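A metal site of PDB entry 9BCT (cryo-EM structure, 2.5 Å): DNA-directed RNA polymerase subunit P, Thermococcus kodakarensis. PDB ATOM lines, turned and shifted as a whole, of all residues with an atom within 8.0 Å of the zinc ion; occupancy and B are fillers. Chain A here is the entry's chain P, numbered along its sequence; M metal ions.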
ATOM      1  N   ARG A   7      21.510 -15.169  23.660  1.00  0.00           N
ATOM      2  CA  ARG A   7      22.547 -15.308  22.634  1.00  0.00           C
ATOM      3  C   ARG A   7      21.958 -15.960  21.396  1.00  0.00           C
ATOM      4  O   ARG A   7      21.222 -16.952  21.503  1.00  0.00           O
ATOM      5  CB  ARG A   7      23.726 -16.130  23.158  1.00  0.00           C
ATOM      6  CG  ARG A   7      24.637 -15.378  24.116  1.00  0.00           C
ATOM      7  CD  ARG A   7      25.367 -14.254  23.407  1.00  0.00           C
ATOM      8  NE  ARG A   7      26.557 -14.725  22.707  1.00  0.00           N
ATOM      9  CZ  ARG A   7      27.725 -14.967  23.292  1.00  0.00           C
ATOM     10  NH1 ARG A   7      27.896 -14.781  24.595  1.00  0.00           N
ATOM     11  NH2 ARG A   7      28.738 -15.401  22.556  1.00  0.00           N
ATOM     12  N   CYS A   8      22.267 -15.410  20.234  1.00  0.00           N
ATOM     13  CA  CYS A   8      21.770 -15.969  18.988  1.00  0.00           C
ATOM     14  C   CYS A   8      22.479 -17.273  18.656  1.00  0.00           C
ATOM     15  O   CYS A   8      23.639 -17.498  19.014  1.00  0.00           O
ATOM     16  CB  CYS A   8      21.952 -14.973  17.836  1.00  0.00           C
ATOM     17  SG  CYS A   8      21.083 -15.454  16.334  1.00  0.00           S
ATOM     18  N   ALA A   9      21.768 -18.158  17.946  1.00  0.00           N
ATOM     19  CA  ALA A   9      22.334 -19.453  17.590  1.00  0.00           C
ATOM     20  C   ALA A   9      23.357 -19.329  16.468  1.00  0.00           C
ATOM     21  O   ALA A   9      24.402 -19.979  16.499  1.00  0.00           O
ATOM     22  CB  ALA A   9      21.218 -20.411  17.194  1.00  0.00           C
ATOM     23  N   LYS A  10      23.078 -18.494  15.461  1.00  0.00           N
ATOM     24  CA  LYS A  10      23.936 -18.397  14.289  1.00  0.00           C
ATOM     25  C   LYS A  10      24.975 -17.289  14.418  1.00  0.00           C
ATOM     26  O   LYS A  10      26.179 -17.561  14.381  1.00  0.00           O
ATOM     27  CB  LYS A  10      23.085 -18.200  13.029  1.00  0.00           C
ATOM     28  CG  LYS A  10      21.644 -18.654  13.179  1.00  0.00           C
ATOM     29  CD  LYS A  10      21.445 -20.044  12.591  1.00  0.00           C
ATOM     30  CE  LYS A  10      20.152 -20.669  13.080  1.00  0.00           C
ATOM     31  NZ  LYS A  10      18.971 -20.209  12.307  1.00  0.00           N
ATOM     32  N   CYS A  11      24.523 -16.048  14.572  1.00  0.00           N
ATOM     33  CA  CYS A  11      25.461 -14.939  14.660  1.00  0.00           C
ATOM     34  C   CYS A  11      26.166 -14.889  16.016  1.00  0.00           C
ATOM     35  O   CYS A  11      27.331 -14.472  16.098  1.00  0.00           O
ATOM     36  CB  CYS A  11      24.755 -13.611  14.386  1.00  0.00           C
ATOM     37  SG  CYS A  11      23.794 -12.957  15.773  1.00  0.00           S
ATOM     38  N   GLY A  12      25.481 -15.309  17.072  1.00  0.00           N
ATOM     39  CA  GLY A  12      26.074 -15.346  18.401  1.00  0.00           C
ATOM     40  C   GLY A  12      26.047 -14.039  19.161  1.00  0.00           C
ATOM     41  O   GLY A  12      26.522 -13.999  20.303  1.00  0.00           O
ATOM     42  N   LYS A  13      25.521 -12.975  18.574  1.00  0.00           N
ATOM     43  CA  LYS A  13      25.450 -11.693  19.259  1.00  0.00           C
ATOM     44  C   LYS A  13      24.345 -11.705  20.306  1.00  0.00           C
ATOM     45  O   LYS A  13      23.387 -12.484  20.225  1.00  0.00           O
ATOM     46  CB  LYS A  13      25.230 -10.559  18.260  1.00  0.00           C
ATOM     47  CG  LYS A  13      26.382 -10.361  17.286  1.00  0.00           C
ATOM     48  CD  LYS A  13      26.334  -8.982  16.650  1.00  0.00           C
ATOM     49  CE  LYS A  13      26.364  -9.080  15.128  1.00  0.00           C
ATOM     50  NZ  LYS A  13      25.183  -9.805  14.589  1.00  0.00           N
ATOM     51  N   GLU A  14      24.484 -10.825  21.293  1.00  0.00           N
ATOM     52  CA  GLU A  14      23.511 -10.761  22.372  1.00  0.00           C
ATOM     53  C   GLU A  14      22.188 -10.179  21.879  1.00  0.00           C
ATOM     54  O   GLU A  14      22.166  -9.157  21.193  1.00  0.00           O
ATOM     55  CB  GLU A  14      24.058  -9.902  23.518  1.00  0.00           C
ATOM     56  CG  GLU A  14      24.762 -10.705  24.607  1.00  0.00           C
ATOM     57  CD  GLU A  14      26.264 -10.595  24.524  1.00  0.00           C
ATOM     58  OE1 GLU A  14      26.804 -10.528  23.400  1.00  0.00           O
ATOM     59  OE2 GLU A  14      26.921 -10.572  25.594  1.00  0.00           O
ATOM     60  N   VAL A  15      21.084 -10.850  22.219  1.00  0.00           N
ATOM     61  CA  VAL A  15      19.754 -10.442  21.824  1.00  0.00           C
ATOM     62  C   VAL A  15      18.953 -10.158  23.089  1.00  0.00           C
ATOM     63  O   VAL A  15      18.926 -10.984  24.005  1.00  0.00           O
ATOM     64  CB  VAL A  15      19.056 -11.521  20.969  1.00  0.00           C
ATOM     65  CG1 VAL A  15      17.680 -11.054  20.537  1.00  0.00           C
ATOM     66  CG2 VAL A  15      19.915 -11.852  19.753  1.00  0.00           C
ATOM     67  N   ARG A  26      13.040 -13.383  18.080  1.00  0.00           N
ATOM     68  CA  ARG A  26      13.997 -13.611  17.010  1.00  0.00           C
ATOM     69  C   ARG A  26      15.173 -12.661  17.209  1.00  0.00           C
ATOM     70  O   ARG A  26      15.103 -11.711  17.988  1.00  0.00           O
ATOM     71  CB  ARG A  26      13.371 -13.404  15.627  1.00  0.00           C
ATOM     72  CG  ARG A  26      13.304 -11.950  15.198  1.00  0.00           C
ATOM     73  CD  ARG A  26      12.719 -11.808  13.809  1.00  0.00           C
ATOM     74  NE  ARG A  26      13.714 -11.398  12.820  1.00  0.00           N
ATOM     75  CZ  ARG A  26      14.027 -10.131  12.564  1.00  0.00           C
ATOM     76  NH1 ARG A  26      13.440  -9.132  13.187  1.00  0.00           N
ATOM     77  NH2 ARG A  26      14.955  -9.875  11.642  1.00  0.00           N
ATOM     78  N   CYS A  27      16.254 -12.940  16.486  1.00  0.00           N
ATOM     79  CA  CYS A  27      17.405 -12.045  16.494  1.00  0.00           C
ATOM     80  C   CYS A  27      17.235 -10.997  15.410  1.00  0.00           C
ATOM     81  O   CYS A  27      17.249 -11.348  14.223  1.00  0.00           O
ATOM     82  CB  CYS A  27      18.697 -12.827  16.275  1.00  0.00           C
ATOM     83  SG  CYS A  27      20.152 -11.791  16.015  1.00  0.00           S
ATOM     84  N   PRO A  28      17.077  -9.721  15.754  1.00  0.00           N
ATOM     85  CA  PRO A  28      16.923  -8.687  14.710  1.00  0.00           C
ATOM     86  C   PRO A  28      18.175  -8.471  13.888  1.00  0.00           C
ATOM     87  O   PRO A  28      18.082  -7.887  12.800  1.00  0.00           O
ATOM     88  CB  PRO A  28      16.556  -7.437  15.512  1.00  0.00           C
ATOM     89  CG  PRO A  28      17.151  -7.669  16.858  1.00  0.00           C
ATOM     90  CD  PRO A  28      17.056  -9.143  17.110  1.00  0.00           C
ATOM     91  N   TYR A  29      19.339  -8.924  14.351  1.00  0.00           N
ATOM     92  CA  TYR A  29      20.590  -8.629  13.659  1.00  0.00           C
ATOM     93  C   TYR A  29      20.717  -9.445  12.382  1.00  0.00           C
ATOM     94  O   TYR A  29      21.155  -8.932  11.347  1.00  0.00           O
ATOM     95  CB  TYR A  29      21.788  -8.873  14.581  1.00  0.00           C
ATOM     96  CG  TYR A  29      21.802  -8.163  15.938  1.00  0.00           C
ATOM     97  CD1 TYR A  29      22.862  -8.326  16.807  1.00  0.00           C
ATOM     98  CD2 TYR A  29      20.779  -7.281  16.321  1.00  0.00           C
ATOM     99  CE1 TYR A  29      22.894  -7.692  18.035  1.00  0.00           C
ATOM    100  CE2 TYR A  29      20.807  -6.648  17.540  1.00  0.00           C
ATOM    101  CZ  TYR A  29      21.865  -6.843  18.394  1.00  0.00           C
ATOM    102  OH  TYR A  29      21.889  -6.197  19.612  1.00  0.00           O
ATOM    103  N   CYS A  30      20.340 -10.726  12.434  1.00  0.00           N
ATOM    104  CA  CYS A  30      20.459 -11.604  11.277  1.00  0.00           C
ATOM    105  C   CYS A  30      19.152 -12.309  10.907  1.00  0.00           C
ATOM    106  O   CYS A  30      19.147 -13.097   9.959  1.00  0.00           O
ATOM    107  CB  CYS A  30      21.553 -12.652  11.506  1.00  0.00           C
ATOM    108  SG  CYS A  30      21.295 -13.700  12.944  1.00  0.00           S
ATOM    109  N   GLY A  31      18.065 -12.054  11.627  1.00  0.00           N
ATOM    110  CA  GLY A  31      16.794 -12.678  11.335  1.00  0.00           C
ATOM    111  C   GLY A  31      16.631 -14.086  11.866  1.00  0.00           C
ATOM    112  O   GLY A  31      15.598 -14.713  11.596  1.00  0.00           O
ATOM    113  N   SER A  32      17.600 -14.596  12.617  1.00  0.00           N
ATOM    114  CA  SER A  32      17.511 -15.959  13.147  1.00  0.00           C
ATOM    115  C   SER A  32      16.416 -16.048  14.205  1.00  0.00           C
ATOM    116  O   SER A  32      16.276 -15.172  15.057  1.00  0.00           O
ATOM    117  CB  SER A  32      18.849 -16.389  13.735  1.00  0.00           C
ATOM    118  OG  SER A  32      18.670 -17.282  14.819  1.00  0.00           O
ATOM    119  N   LYS A  33      15.660 -17.136  14.149  1.00  0.00           N
ATOM    120  CA  LYS A  33      14.519 -17.349  15.031  1.00  0.00           C
ATOM    121  C   LYS A  33      14.850 -18.271  16.202  1.00  0.00           C
ATOM    122  O   LYS A  33      13.956 -18.608  16.979  1.00  0.00           O
ATOM    123  CB  LYS A  33      13.351 -17.924  14.226  1.00  0.00           C
ATOM    124  CG  LYS A  33      12.971 -17.059  13.035  1.00  0.00           C
ATOM    125  CD  LYS A  33      11.678 -16.293  13.246  1.00  0.00           C
ATOM    126  CE  LYS A  33      10.605 -17.171  13.841  1.00  0.00           C
ATOM    127  NZ  LYS A  33       9.387 -16.386  14.204  1.00  0.00           N
ATOM    128  N   ILE A  34      16.106 -18.672  16.349  1.00  0.00           N
ATOM    129  CA  ILE A  34      16.555 -19.589  17.393  1.00  0.00           C
ATOM    130  C   ILE A  34      17.555 -18.854  18.267  1.00  0.00           C
ATOM    131  O   ILE A  34      18.532 -18.280  17.761  1.00  0.00           O
ATOM    132  CB  ILE A  34      17.163 -20.864  16.798  1.00  0.00           C
ATOM    133  CG1 ILE A  34      16.121 -21.618  15.960  1.00  0.00           C
ATOM    134  CG2 ILE A  34      17.720 -21.758  17.888  1.00  0.00           C
ATOM    135  CD1 ILE A  34      16.726 -22.507  14.898  1.00  0.00           C
ATOM    136  N   LEU A  35      17.330 -18.873  19.580  1.00  0.00           N
ATOM    137  CA  LEU A  35      18.184 -18.178  20.533  1.00  0.00           C
ATOM    138  C   LEU A  35      18.651 -19.138  21.613  1.00  0.00           C
ATOM    139  O   LEU A  35      18.001 -20.139  21.928  1.00  0.00           O
ATOM    140  CB  LEU A  35      17.452 -16.990  21.185  1.00  0.00           C
ATOM    141  CG  LEU A  35      16.952 -15.883  20.259  1.00  0.00           C
ATOM    142  CD1 LEU A  35      16.406 -14.723  21.076  1.00  0.00           C
ATOM    143  CD2 LEU A  35      18.067 -15.410  19.335  1.00  0.00           C
HETATM  144 ZN    ZN M   1      21.581 -13.462  15.244  1.00  0.00          ZN
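OG of Ser 32 lies close to SG of Cys 8, 3.4 Å away. N of Cys 8 is in hydrogen-bond range of O of Lys 13, at 3.1 Å. The backbone NH (N) of Lys 10 sits close to the side-chain sulfur (SG) of Cys 8 (3.7 Å). The backbone NH (N) of Cys 27 is in hydrogen-bond range of the backbone carbonyl oxygen (O) of Ser 32 (2.7 Å). The side-chain sulfur (SG) of Cys 27 lies close to the backbone NH (N) of Tyr 29. SG of Cys 11 lies close to N of Lys 13 (3.3 Å).
Of the 19 residues printed, 4 come within 4 Å of the zinc ion.
The zinc ion is bound by the side-chain sulfur of Cys 8 (2.3 Å), the side-chain sulfur of Cys 27 (2.3 Å), the side-chain sulfur of Cys 30 (2.3 Å) and the side-chain sulfur of Cys 11 (2.3 Å). The zinc ion has four donor atoms within binding distance.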
